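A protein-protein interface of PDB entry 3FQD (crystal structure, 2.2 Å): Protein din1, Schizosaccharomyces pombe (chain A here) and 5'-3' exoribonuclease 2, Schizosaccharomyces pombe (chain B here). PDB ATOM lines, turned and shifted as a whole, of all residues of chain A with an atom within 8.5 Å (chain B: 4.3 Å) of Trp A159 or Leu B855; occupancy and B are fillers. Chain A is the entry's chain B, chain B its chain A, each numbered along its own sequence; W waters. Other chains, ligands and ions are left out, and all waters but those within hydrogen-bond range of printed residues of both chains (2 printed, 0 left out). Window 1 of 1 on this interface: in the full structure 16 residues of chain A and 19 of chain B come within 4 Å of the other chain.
NZ of Lys B851 lies within hydrogen-bond range of O of Trp A159, 2.7 Å away. The side-chain amino group of Lys B851 lies within hydrogen-bond range of the backbone carbonyl oxygen of Asp A160, at 3.5 Å. NZ of Lys B851 is in hydrogen-bond range of O of Cys A162 (2.7 Å). The side-chain sulfur (SD) of Met B853 sits at hydrogen-bond distance from the indole nitrogen (NE1) of Trp A159 (3.7 Å). The backbone carbonyl oxygen (O) of Leu B854 is in hydrogen-bond range of the side-chain hydroxyl (OH) of Tyr A46 (2.5 Å). The guanidinium group (NE) of Arg B856 is in hydrogen-bond range of the backbone carbonyl oxygen (O) of Trp A204 (2.8 Å).
OE2 of Glu B250 lies within salt-bridge range of NH1 of Arg B221, at 2.9 Å. NE of Arg B221 lies within hydrogen-bond range of NE2 of His B850. The backbone carbonyl oxygen (O) of Pro A47 is in hydrogen-bond range of the guanidinium group (NH2) of Arg A170 (3.2 Å). The backbone carbonyl oxygen of Glu A157 is in hydrogen-bond range of the side-chain sulfur of Cys A162. The backbone NH of Gln A166 sits at hydrogen-bond distance from the side-chain hydroxyl of Ser A163 (3.1 Å). The guanidinium group of Arg A170 is in hydrogen-bond range of the backbone carbonyl oxygen of Ile A167, 3.0 Å away.
Among the printed residues, merely in contact across the chains: Tyr A45 with Arg B856 (3.5 Å), Tyr A46 with Met B853 (3.5 Å), Tyr A46 with Arg B856 (3.7 Å), Pro A47 with Arg B856 (3.5 Å), Trp A159 with Arg B221 (3.5 Å), Trp A159 with His B850 (3.98 Å), Trp A159 with Leu B855 (3.9 Å), Ser A163 with Lys B851 (3.98 Å), Arg A164 with Lys B851 (3.6 Å), Arg A164 with Met B853 (3.6 Å), Ile A167 with Lys B851 (3.7 Å), Ile A167 with Met B853 (3.9 Å), Trp A204 with Gly B857 (3.6 Å) and Glu A288 with Gly B857 (3.3 Å).
Of the printed residues of chain B, Ser A163 touches Lys B851. Of the printed residues of chain B, Arg A164 touches Lys B851 and Met B853. Of the printed residues of chain A, Met B853 touches Tyr A46 (3.5 Å), Trp A159 (3.7 Å), Arg A164 (3.6 Å) and Ile A167 (3.9 Å). Of chain A, only Trp A159 comes within 4 Å of Leu B855. The nearest residue of chain A that does not touch Leu B855 is Tyr A46 (4.2 Å). The nearest printed residue of chain A that does not touch Arg B856 is Asp A205 (4.01 Å).
Of the 21 printed residues of chain A, 11 touch a printed residue of chain B. Printed residues of chain A that touch a printed residue of chain B: Tyr A45, Tyr A46, Pro A47, Trp A159, Asp A160, Cys A162, Ser A163, Arg A164, Ile A167, Trp A204 and Glu A288. Hydrophobic or aromatic side chains of chain A that line the printed part of chain B: Tyr A45, Tyr A46, Pro A47, Trp A159, Ile A167 and Trp A204. Of the 12 printed residues of chain B, 8 touch a printed residue of chain A. Hydrophobic or aromatic side chains of chain B that line the printed part of chain A: His B850, Met B853 and Leu B855. Among the printed residues, no Asp or Glu carboxylate lies within 4 Å of a Lys or Arg side-chain nitrogen of the other chain.
Water W1 bridges the side-chain carboxylate (OD1) of Asp A160 and the side-chain amino group (NZ) of Lys B851. Water W2 bridges the backbone carbonyl oxygen of Gly B857 and the side-chain carboxylate of Glu A288.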
ATOM      1  N   TYR A  44      -1.880 -37.566  19.431  1.00  0.00           N
ATOM      2  CA  TYR A  44      -1.113 -36.542  18.727  1.00  0.00           C
ATOM      3  C   TYR A  44       0.338 -36.578  19.169  1.00  0.00           C
ATOM      4  O   TYR A  44       0.635 -36.800  20.349  1.00  0.00           O
ATOM      5  CB  TYR A  44      -1.721 -35.154  18.970  1.00  0.00           C
ATOM      6  CG  TYR A  44      -3.175 -35.072  18.567  1.00  0.00           C
ATOM      7  CD1 TYR A  44      -4.178 -35.600  19.385  1.00  0.00           C
ATOM      8  CD2 TYR A  44      -3.550 -34.491  17.366  1.00  0.00           C
ATOM      9  CE1 TYR A  44      -5.514 -35.543  19.018  1.00  0.00           C
ATOM     10  CE2 TYR A  44      -4.886 -34.423  16.992  1.00  0.00           C
ATOM     11  CZ  TYR A  44      -5.862 -34.950  17.823  1.00  0.00           C
ATOM     12  OH  TYR A  44      -7.184 -34.887  17.456  1.00  0.00           O
ATOM     13  N   TYR A  45       1.241 -36.364  18.219  1.00  0.00           N
ATOM     14  CA  TYR A  45       2.662 -36.401  18.518  1.00  0.00           C
ATOM     15  C   TYR A  45       3.125 -35.170  19.301  1.00  0.00           C
ATOM     16  O   TYR A  45       2.941 -34.030  18.863  1.00  0.00           O
ATOM     17  CB  TYR A  45       3.486 -36.574  17.233  1.00  0.00           C
ATOM     18  CG  TYR A  45       4.977 -36.461  17.450  1.00  0.00           C
ATOM     19  CD1 TYR A  45       5.685 -37.462  18.132  1.00  0.00           C
ATOM     20  CD2 TYR A  45       5.683 -35.350  16.990  1.00  0.00           C
ATOM     21  CE1 TYR A  45       7.055 -37.354  18.344  1.00  0.00           C
ATOM     22  CE2 TYR A  45       7.052 -35.235  17.196  1.00  0.00           C
ATOM     23  CZ  TYR A  45       7.730 -36.238  17.874  1.00  0.00           C
ATOM     24  OH  TYR A  45       9.082 -36.123  18.064  1.00  0.00           O
ATOM     25  N   TYR A  46       3.719 -35.416  20.465  1.00  0.00           N
ATOM     26  CA  TYR A  46       4.489 -34.393  21.177  1.00  0.00           C
ATOM     27  C   TYR A  46       5.651 -35.048  21.925  1.00  0.00           C
ATOM     28  O   TYR A  46       5.425 -35.890  22.795  1.00  0.00           O
ATOM     29  CB  TYR A  46       3.619 -33.549  22.127  1.00  0.00           C
ATOM     30  CG  TYR A  46       4.342 -32.298  22.587  1.00  0.00           C
ATOM     31  CD1 TYR A  46       4.489 -31.201  21.733  1.00  0.00           C
ATOM     32  CD2 TYR A  46       4.923 -32.231  23.852  1.00  0.00           C
ATOM     33  CE1 TYR A  46       5.184 -30.063  22.131  1.00  0.00           C
ATOM     34  CE2 TYR A  46       5.619 -31.094  24.261  1.00  0.00           C
ATOM     35  CZ  TYR A  46       5.742 -30.016  23.396  1.00  0.00           C
ATOM     36  OH  TYR A  46       6.435 -28.897  23.795  1.00  0.00           O
ATOM     37  N   PRO A  47       6.883 -34.644  21.601  1.00  0.00           N
ATOM     38  CA  PRO A  47       8.088 -35.357  22.038  1.00  0.00           C
ATOM     39  C   PRO A  47       8.345 -35.307  23.550  1.00  0.00           C
ATOM     40  O   PRO A  47       7.897 -34.378  24.222  1.00  0.00           O
ATOM     41  CB  PRO A  47       9.210 -34.627  21.288  1.00  0.00           C
ATOM     42  CG  PRO A  47       8.675 -33.243  21.088  1.00  0.00           C
ATOM     43  CD  PRO A  47       7.219 -33.448  20.807  1.00  0.00           C
ATOM     44  N   LEU A 155      -0.083 -37.389  22.917  1.00  0.00           N
ATOM     45  CA  LEU A 155      -1.059 -36.661  23.726  1.00  0.00           C
ATOM     46  C   LEU A 155      -2.494 -37.062  23.326  1.00  0.00           C
ATOM     47  O   LEU A 155      -2.725 -37.442  22.181  1.00  0.00           O
ATOM     48  CB  LEU A 155      -0.868 -35.155  23.524  1.00  0.00           C
ATOM     49  CG  LEU A 155       0.420 -34.495  24.014  1.00  0.00           C
ATOM     50  CD1 LEU A 155       0.413 -33.008  23.636  1.00  0.00           C
ATOM     51  CD2 LEU A 155       0.592 -34.670  25.530  1.00  0.00           C
ATOM     52  N   PRO A 156      -3.450 -36.993  24.257  1.00  0.00           N
ATOM     53  CA  PRO A 156      -4.853 -37.289  23.941  1.00  0.00           C
ATOM     54  C   PRO A 156      -5.540 -36.207  23.099  1.00  0.00           C
ATOM     55  O   PRO A 156      -6.583 -36.470  22.497  1.00  0.00           O
ATOM     56  CB  PRO A 156      -5.512 -37.366  25.323  1.00  0.00           C
ATOM     57  CG  PRO A 156      -4.684 -36.444  26.172  1.00  0.00           C
ATOM     58  CD  PRO A 156      -3.269 -36.673  25.687  1.00  0.00           C
ATOM     59  N   GLU A 157      -4.970 -35.003  23.089  1.00  0.00           N
ATOM     60  CA  GLU A 157      -5.494 -33.872  22.324  1.00  0.00           C
ATOM     61  C   GLU A 157      -4.325 -33.132  21.679  1.00  0.00           C
ATOM     62  O   GLU A 157      -3.167 -33.488  21.900  1.00  0.00           O
ATOM     63  CB  GLU A 157      -6.289 -32.911  23.224  1.00  0.00           C
ATOM     64  CG  GLU A 157      -7.466 -33.521  23.984  1.00  0.00           C
ATOM     65  CD  GLU A 157      -8.577 -34.055  23.084  1.00  0.00           C
ATOM     66  OE1 GLU A 157      -8.692 -33.623  21.907  1.00  0.00           O
ATOM     67  OE2 GLU A 157      -9.349 -34.920  23.563  1.00  0.00           O
ATOM     68  N   ILE A 158      -4.625 -32.117  20.874  1.00  0.00           N
ATOM     69  CA  ILE A 158      -3.577 -31.266  20.317  1.00  0.00           C
ATOM     70  C   ILE A 158      -2.831 -30.555  21.448  1.00  0.00           C
ATOM     71  O   ILE A 158      -3.375 -30.358  22.539  1.00  0.00           O
ATOM     72  CB  ILE A 158      -4.138 -30.246  19.282  1.00  0.00           C
ATOM     73  CG1 ILE A 158      -5.112 -29.257  19.949  1.00  0.00           C
ATOM     74  CG2 ILE A 158      -4.775 -30.982  18.082  1.00  0.00           C
ATOM     75  CD1 ILE A 158      -5.484 -28.064  19.085  1.00  0.00           C
ATOM     76  N   TRP A 159      -1.585 -30.184  21.177  1.00  0.00           N
ATOM     77  CA  TRP A 159      -0.700 -29.570  22.159  1.00  0.00           C
ATOM     78  C   TRP A 159      -1.362 -28.446  22.965  1.00  0.00           C
ATOM     79  O   TRP A 159      -1.269 -28.422  24.192  1.00  0.00           O
ATOM     80  CB  TRP A 159       0.570 -29.074  21.454  1.00  0.00           C
ATOM     81  CG  TRP A 159       1.460 -28.245  22.311  1.00  0.00           C
ATOM     82  CD1 TRP A 159       2.347 -28.694  23.250  1.00  0.00           C
ATOM     83  CD2 TRP A 159       1.551 -26.816  22.323  1.00  0.00           C
ATOM     84  NE1 TRP A 159       2.988 -27.631  23.840  1.00  0.00           N
ATOM     85  CE2 TRP A 159       2.517 -26.464  23.294  1.00  0.00           C
ATOM     86  CE3 TRP A 159       0.914 -25.791  21.608  1.00  0.00           C
ATOM     87  CZ2 TRP A 159       2.861 -25.141  23.568  1.00  0.00           C
ATOM     88  CZ3 TRP A 159       1.257 -24.474  21.878  1.00  0.00           C
ATOM     89  CH2 TRP A 159       2.223 -24.161  22.854  1.00  0.00           C
ATOM     90  N   ASP A 160      -2.040 -27.532  22.272  1.00  0.00           N
ATOM     91  CA  ASP A 160      -2.648 -26.368  22.910  1.00  0.00           C
ATOM     92  C   ASP A 160      -3.794 -26.717  23.860  1.00  0.00           C
ATOM     93  O   ASP A 160      -4.012 -26.021  24.854  1.00  0.00           O
ATOM     94  CB  ASP A 160      -3.137 -25.373  21.858  1.00  0.00           C
ATOM     95  CG  ASP A 160      -3.581 -24.058  22.463  1.00  0.00           C
ATOM     96  OD1 ASP A 160      -2.821 -23.474  23.268  1.00  0.00           O
ATOM     97  OD2 ASP A 160      -4.674 -23.524  22.185  1.00  0.00           O
ATOM     98  N   ALA A 161      -4.518 -27.787  23.539  1.00  0.00           N
ATOM     99  CA  ALA A 161      -5.657 -28.241  24.339  1.00  0.00           C
ATOM    100  C   ALA A 161      -5.243 -29.063  25.565  1.00  0.00           C
ATOM    101  O   ALA A 161      -6.083 -29.402  26.399  1.00  0.00           O
ATOM    102  CB  ALA A 161      -6.634 -29.031  23.468  1.00  0.00           C
ATOM    103  N   CYS A 162      -3.952 -29.373  25.673  1.00  0.00           N
ATOM    104  CA  CYS A 162      -3.427 -30.132  26.807  1.00  0.00           C
ATOM    105  C   CYS A 162      -2.790 -29.240  27.864  1.00  0.00           C
ATOM    106  O   CYS A 162      -2.041 -28.323  27.535  1.00  0.00           O
ATOM    107  CB  CYS A 162      -2.393 -31.143  26.328  1.00  0.00           C
ATOM    108  SG  CYS A 162      -3.094 -32.474  25.353  1.00  0.00           S
ATOM    109  N   SER A 163      -3.069 -29.524  29.133  1.00  0.00           N
ATOM    110  CA  SER A 163      -2.424 -28.798  30.226  1.00  0.00           C
ATOM    111  C   SER A 163      -0.940 -29.151  30.236  1.00  0.00           C
ATOM    112  O   SER A 163      -0.545 -30.165  29.656  1.00  0.00           O
ATOM    113  CB  SER A 163      -3.064 -29.164  31.568  1.00  0.00           C
ATOM    114  OG  SER A 163      -2.751 -30.499  31.931  1.00  0.00           O
ATOM    115  N   ARG A 164      -0.107 -28.335  30.879  1.00  0.00           N
ATOM    116  CA  ARG A 164       1.309 -28.693  30.951  1.00  0.00           C
ATOM    117  C   ARG A 164       1.571 -29.907  31.869  1.00  0.00           C
ATOM    118  O   ARG A 164       2.473 -30.690  31.605  1.00  0.00           O
ATOM    119  CB  ARG A 164       2.232 -27.478  31.197  1.00  0.00           C
ATOM    120  CG  ARG A 164       2.652 -27.190  32.607  1.00  0.00           C
ATOM    121  CD  ARG A 164       4.046 -26.545  32.732  1.00  0.00           C
ATOM    122  NE  ARG A 164       4.281 -25.452  31.784  1.00  0.00           N
ATOM    123  CZ  ARG A 164       5.328 -25.366  30.958  1.00  0.00           C
ATOM    124  NH1 ARG A 164       6.269 -26.304  30.953  1.00  0.00           N
ATOM    125  NH2 ARG A 164       5.439 -24.330  30.137  1.00  0.00           N
ATOM    126  N   GLN A 166      -0.459 -32.526  32.064  1.00  0.00           N
ATOM    127  CA  GLN A 166      -0.785 -33.632  31.165  1.00  0.00           C
ATOM    128  C   GLN A 166       0.434 -34.073  30.358  1.00  0.00           C
ATOM    129  O   GLN A 166       0.683 -35.270  30.191  1.00  0.00           O
ATOM    130  CB  GLN A 166      -1.884 -33.186  30.202  1.00  0.00           C
ATOM    131  CG  GLN A 166      -3.087 -34.098  30.132  1.00  0.00           C
ATOM    132  CD  GLN A 166      -4.313 -33.419  29.524  1.00  0.00           C
ATOM    133  OE1 GLN A 166      -4.517 -32.213  29.687  1.00  0.00           O
ATOM    134  NE2 GLN A 166      -5.133 -34.198  28.835  1.00  0.00           N
ATOM    135  N   ILE A 167       1.182 -33.092  29.856  1.00  0.00           N
ATOM    136  CA  ILE A 167       2.369 -33.332  29.050  1.00  0.00           C
ATOM    137  C   ILE A 167       3.543 -33.812  29.910  1.00  0.00           C
ATOM    138  O   ILE A 167       4.243 -34.763  29.544  1.00  0.00           O
ATOM    139  CB  ILE A 167       2.750 -32.049  28.260  1.00  0.00           C
ATOM    140  CG1 ILE A 167       1.618 -31.650  27.301  1.00  0.00           C
ATOM    141  CG2 ILE A 167       4.077 -32.234  27.520  1.00  0.00           C
ATOM    142  CD1 ILE A 167       1.769 -30.270  26.691  1.00  0.00           C
ATOM    143  N   ARG A 170       3.632 -37.586  31.733  1.00  0.00           N
ATOM    144  CA  ARG A 170       3.521 -38.766  30.857  1.00  0.00           C
ATOM    145  C   ARG A 170       4.437 -39.928  31.243  1.00  0.00           C
ATOM    146  O   ARG A 170       4.106 -41.085  30.985  1.00  0.00           O
ATOM    147  CB  ARG A 170       3.719 -38.387  29.386  1.00  0.00           C
ATOM    148  CG  ARG A 170       2.510 -37.697  28.775  1.00  0.00           C
ATOM    149  CD  ARG A 170       2.672 -37.304  27.325  1.00  0.00           C
ATOM    150  NE  ARG A 170       3.781 -36.375  27.104  1.00  0.00           N
ATOM    151  CZ  ARG A 170       4.286 -36.085  25.909  1.00  0.00           C
ATOM    152  NH1 ARG A 170       3.789 -36.652  24.819  1.00  0.00           N
ATOM    153  NH2 ARG A 170       5.299 -35.237  25.801  1.00  0.00           N
ATOM    154  N   ILE A 203      -0.930 -38.826  15.216  1.00  0.00           N
ATOM    155  CA  ILE A 203      -0.974 -37.908  14.089  1.00  0.00           C
ATOM    156  C   ILE A 203      -0.108 -36.680  14.355  1.00  0.00           C
ATOM    157  O   ILE A 203       0.061 -36.267  15.508  1.00  0.00           O
ATOM    158  CB  ILE A 203      -2.426 -37.531  13.730  1.00  0.00           C
ATOM    159  CG1 ILE A 203      -3.078 -36.730  14.846  1.00  0.00           C
ATOM    160  CG2 ILE A 203      -3.239 -38.790  13.437  1.00  0.00           C
ATOM    161  CD1 ILE A 203      -4.566 -36.538  14.656  1.00  0.00           C
ATOM    162  N   TRP A 204       0.438 -36.119  13.277  1.00  0.00           N
ATOM    163  CA  TRP A 204       1.345 -34.971  13.336  1.00  0.00           C
ATOM    164  C   TRP A 204       0.626 -33.692  13.743  1.00  0.00           C
ATOM    165  O   TRP A 204       1.117 -32.944  14.584  1.00  0.00           O
ATOM    166  CB  TRP A 204       2.013 -34.775  11.975  1.00  0.00           C
ATOM    167  CG  TRP A 204       3.057 -33.686  11.909  1.00  0.00           C
ATOM    168  CD1 TRP A 204       2.931 -32.458  11.316  1.00  0.00           C
ATOM    169  CD2 TRP A 204       4.390 -33.740  12.433  1.00  0.00           C
ATOM    170  NE1 TRP A 204       4.098 -31.743  11.448  1.00  0.00           N
ATOM    171  CE2 TRP A 204       5.014 -32.508  12.126  1.00  0.00           C
ATOM    172  CE3 TRP A 204       5.124 -34.707  13.135  1.00  0.00           C
ATOM    173  CZ2 TRP A 204       6.335 -32.221  12.494  1.00  0.00           C
ATOM    174  CZ3 TRP A 204       6.439 -34.415  13.504  1.00  0.00           C
ATOM    175  CH2 TRP A 204       7.028 -33.185  13.180  1.00  0.00           C
ATOM    176  N   ASP A 205      -0.530 -33.446  13.127  1.00  0.00           N
ATOM    177  CA  ASP A 205      -1.283 -32.209  13.318  1.00  0.00           C
ATOM    178  C   ASP A 205      -2.722 -32.498  13.752  1.00  0.00           C
ATOM    179  O   ASP A 205      -3.024 -32.481  14.943  1.00  0.00           O
ATOM    180  CB  ASP A 205      -1.222 -31.314  12.062  1.00  0.00           C
ATOM    181  CG  ASP A 205      -1.122 -32.108  10.758  1.00  0.00           C
ATOM    182  OD1 ASP A 205      -1.742 -33.198  10.637  1.00  0.00           O
ATOM    183  OD2 ASP A 205      -0.445 -31.703   9.790  1.00  0.00           O
ATOM    184  N   GLU A 288      13.292 -37.317  12.665  1.00  0.00           N
ATOM    185  CA  GLU A 288      12.062 -37.297  11.874  1.00  0.00           C
ATOM    186  C   GLU A 288      12.348 -37.619  10.419  1.00  0.00           C
ATOM    187  O   GLU A 288      13.182 -36.974   9.784  1.00  0.00           O
ATOM    188  CB  GLU A 288      11.382 -35.928  11.937  1.00  0.00           C
ATOM    189  CG  GLU A 288      10.939 -35.487  13.316  1.00  0.00           C
ATOM    190  CD  GLU A 288      10.447 -34.048  13.348  1.00  0.00           C
ATOM    191  OE1 GLU A 288      10.228 -33.436  12.268  1.00  0.00           O
ATOM    192  OE2 GLU A 288      10.278 -33.532  14.468  1.00  0.00           O
ATOM    193  N   ARG B 221       0.809 -20.138  16.342  1.00  0.00           N
ATOM    194  CA  ARG B 221       1.569 -21.223  17.001  1.00  0.00           C
ATOM    195  C   ARG B 221       0.703 -22.365  17.499  1.00  0.00           C
ATOM    196  O   ARG B 221       1.122 -23.527  17.554  1.00  0.00           O
ATOM    197  CB  ARG B 221       2.279 -20.668  18.231  1.00  0.00           C
ATOM    198  CG  ARG B 221       3.646 -20.164  17.976  1.00  0.00           C
ATOM    199  CD  ARG B 221       4.303 -19.546  19.196  1.00  0.00           C
ATOM    200  NE  ARG B 221       4.154 -20.345  20.413  1.00  0.00           N
ATOM    201  CZ  ARG B 221       5.018 -21.260  20.840  1.00  0.00           C
ATOM    202  NH1 ARG B 221       6.112 -21.539  20.149  1.00  0.00           N
ATOM    203  NH2 ARG B 221       4.776 -21.906  21.967  1.00  0.00           N
ATOM    204  N   TYR B 226       0.230 -25.285  11.799  1.00  0.00           N
ATOM    205  CA  TYR B 226       1.234 -24.231  11.781  1.00  0.00           C
ATOM    206  C   TYR B 226       2.626 -24.811  11.572  1.00  0.00           C
ATOM    207  O   TYR B 226       2.956 -25.849  12.139  1.00  0.00           O
ATOM    208  CB  TYR B 226       1.178 -23.482  13.101  1.00  0.00           C
ATOM    209  CG  TYR B 226       2.239 -22.439  13.324  1.00  0.00           C
ATOM    210  CD1 TYR B 226       2.173 -21.206  12.688  1.00  0.00           C
ATOM    211  CD2 TYR B 226       3.286 -22.670  14.209  1.00  0.00           C
ATOM    212  CE1 TYR B 226       3.137 -20.229  12.919  1.00  0.00           C
ATOM    213  CE2 TYR B 226       4.249 -21.699  14.449  1.00  0.00           C
ATOM    214  CZ  TYR B 226       4.164 -20.482  13.797  1.00  0.00           C
ATOM    215  OH  TYR B 226       5.108 -19.518  14.026  1.00  0.00           O
ATOM    216  N   PRO B 228       6.147 -25.260  12.418  1.00  0.00           N
ATOM    217  CA  PRO B 228       6.925 -25.087  13.651  1.00  0.00           C
ATOM    218  C   PRO B 228       8.333 -24.523  13.411  1.00  0.00           C
ATOM    219  O   PRO B 228       9.056 -24.244  14.376  1.00  0.00           O
ATOM    220  CB  PRO B 228       7.009 -26.510  14.210  1.00  0.00           C
ATOM    221  CG  PRO B 228       6.934 -27.391  12.998  1.00  0.00           C
ATOM    222  CD  PRO B 228       6.001 -26.685  12.058  1.00  0.00           C
ATOM    223  N   GLU B 250       9.541 -19.121  19.991  1.00  0.00           N
ATOM    224  CA  GLU B 250       9.866 -19.470  18.622  1.00  0.00           C
ATOM    225  C   GLU B 250      11.354 -19.180  18.464  1.00  0.00           C
ATOM    226  O   GLU B 250      11.765 -18.019  18.439  1.00  0.00           O
ATOM    227  CB  GLU B 250       9.059 -18.626  17.636  1.00  0.00           C
ATOM    228  CG  GLU B 250       7.559 -18.814  17.720  1.00  0.00           C
ATOM    229  CD  GLU B 250       7.073 -19.940  16.839  1.00  0.00           C
ATOM    230  OE1 GLU B 250       7.061 -19.755  15.598  1.00  0.00           O
ATOM    231  OE2 GLU B 250       6.702 -21.002  17.391  1.00  0.00           O
ATOM    232  N   HIS B 850      -1.793 -20.255  26.964  1.00  0.00           N
ATOM    233  CA  HIS B 850      -0.681 -20.524  26.066  1.00  0.00           C
ATOM    234  C   HIS B 850       0.539 -20.967  26.867  1.00  0.00           C
ATOM    235  O   HIS B 850       0.954 -20.286  27.815  1.00  0.00           O
ATOM    236  CB  HIS B 850      -0.363 -19.308  25.194  1.00  0.00           C
ATOM    237  CG  HIS B 850       0.666 -19.587  24.144  1.00  0.00           C
ATOM    238  ND1 HIS B 850       1.990 -19.238  24.289  1.00  0.00           N
ATOM    239  CD2 HIS B 850       0.571 -20.220  22.949  1.00  0.00           C
ATOM    240  CE1 HIS B 850       2.665 -19.630  23.224  1.00  0.00           C
ATOM    241  NE2 HIS B 850       1.827 -20.229  22.395  1.00  0.00           N
ATOM    242  N   LYS B 851       1.097 -22.119  26.499  1.00  0.00           N
ATOM    243  CA  LYS B 851       2.208 -22.697  27.255  1.00  0.00           C
ATOM    244  C   LYS B 851       3.563 -22.262  26.711  1.00  0.00           C
ATOM    245  O   LYS B 851       3.771 -22.191  25.500  1.00  0.00           O
ATOM    246  CB  LYS B 851       2.102 -24.229  27.330  1.00  0.00           C
ATOM    247  CG  LYS B 851       0.880 -24.728  28.103  1.00  0.00           C
ATOM    248  CD  LYS B 851       0.718 -26.249  28.074  1.00  0.00           C
ATOM    249  CE  LYS B 851       0.550 -26.816  26.664  1.00  0.00           C
ATOM    250  NZ  LYS B 851      -0.759 -26.475  26.039  1.00  0.00           N
ATOM    251  N   MET B 853       6.454 -23.463  25.836  1.00  0.00           N
ATOM    252  CA  MET B 853       7.122 -24.689  25.410  1.00  0.00           C
ATOM    253  C   MET B 853       7.427 -24.602  23.930  1.00  0.00           C
ATOM    254  O   MET B 853       6.772 -23.866  23.198  1.00  0.00           O
ATOM    255  CB  MET B 853       6.232 -25.916  25.641  1.00  0.00           C
ATOM    256  CG  MET B 853       5.484 -25.948  26.952  1.00  0.00           C
ATOM    257  SD  MET B 853       4.554 -27.642  27.214  1.00  0.00           S
ATOM    258  CE  MET B 853       6.086 -28.843  27.362  1.00  0.00           C
ATOM    259  N   LEU B 854       8.424 -25.363  23.492  1.00  0.00           N
ATOM    260  CA  LEU B 854       8.715 -25.498  22.079  1.00  0.00           C
ATOM    261  C   LEU B 854       7.665 -26.385  21.415  1.00  0.00           C
ATOM    262  O   LEU B 854       7.174 -27.340  22.021  1.00  0.00           O
ATOM    263  CB  LEU B 854      10.116 -26.086  21.859  1.00  0.00           C
ATOM    264  CG  LEU B 854      11.356 -25.350  22.382  1.00  0.00           C
ATOM    265  CD1 LEU B 854      12.603 -26.169  22.078  1.00  0.00           C
ATOM    266  CD2 LEU B 854      11.489 -23.939  21.813  1.00  0.00           C
ATOM    267  N   LEU B 855       7.321 -26.057  20.174  1.00  0.00           N
ATOM    268  CA  LEU B 855       6.415 -26.880  19.379  1.00  0.00           C
ATOM    269  C   LEU B 855       7.108 -28.166  18.944  1.00  0.00           C
ATOM    270  O   LEU B 855       8.329 -28.200  18.807  1.00  0.00           O
ATOM    271  CB  LEU B 855       5.948 -26.114  18.139  1.00  0.00           C
ATOM    272  CG  LEU B 855       5.244 -24.768  18.347  1.00  0.00           C
ATOM    273  CD1 LEU B 855       5.007 -24.096  17.000  1.00  0.00           C
ATOM    274  CD2 LEU B 855       3.939 -24.908  19.136  1.00  0.00           C
ATOM    275  N   ARG B 856       6.334 -29.225  18.727  1.00  0.00           N
ATOM    276  CA  ARG B 856       6.884 -30.420  18.095  1.00  0.00           C
ATOM    277  C   ARG B 856       7.303 -30.091  16.654  1.00  0.00           C
ATOM    278  O   ARG B 856       6.708 -29.217  16.009  1.00  0.00           O
ATOM    279  CB  ARG B 856       5.885 -31.584  18.139  1.00  0.00           C
ATOM    280  CG  ARG B 856       4.578 -31.366  17.378  1.00  0.00           C
ATOM    281  CD  ARG B 856       4.618 -31.816  15.926  1.00  0.00           C
ATOM    282  NE  ARG B 856       3.393 -31.448  15.228  1.00  0.00           N
ATOM    283  CZ  ARG B 856       3.143 -30.249  14.710  1.00  0.00           C
ATOM    284  NH1 ARG B 856       4.039 -29.271  14.792  1.00  0.00           N
ATOM    285  NH2 ARG B 856       1.987 -30.026  14.100  1.00  0.00           N
ATOM    286  N   GLY B 857       8.335 -30.778  16.173  1.00  0.00           N
ATOM    287  CA  GLY B 857       8.819 -30.584  14.814  1.00  0.00           C
ATOM    288  C   GLY B 857       9.823 -29.457  14.678  1.00  0.00           C
ATOM    289  O   GLY B 857      10.370 -29.235  13.602  1.00  0.00           O
ATOM    290  N   VAL B 858      10.047 -28.746  15.778  1.00  0.00           N
ATOM    291  CA  VAL B 858      11.055 -27.701  15.878  1.00  0.00           C
ATOM    292  C   VAL B 858      12.456 -28.267  15.587  1.00  0.00           C
ATOM    293  O   VAL B 858      12.932 -29.173  16.276  1.00  0.00           O
ATOM    294  CB  VAL B 858      10.957 -26.999  17.275  1.00  0.00           C
ATOM    295  CG1 VAL B 858      12.283 -26.872  17.955  1.00  0.00           C
ATOM    296  CG2 VAL B 858      10.273 -25.653  17.167  1.00  0.00           C
HETATM  297  O   HOH W   1      -0.683 -23.825  24.821  1.00  0.00           O
HETATM  298  O   HOH W   2       9.846 -30.870  11.532  1.00  0.00           O
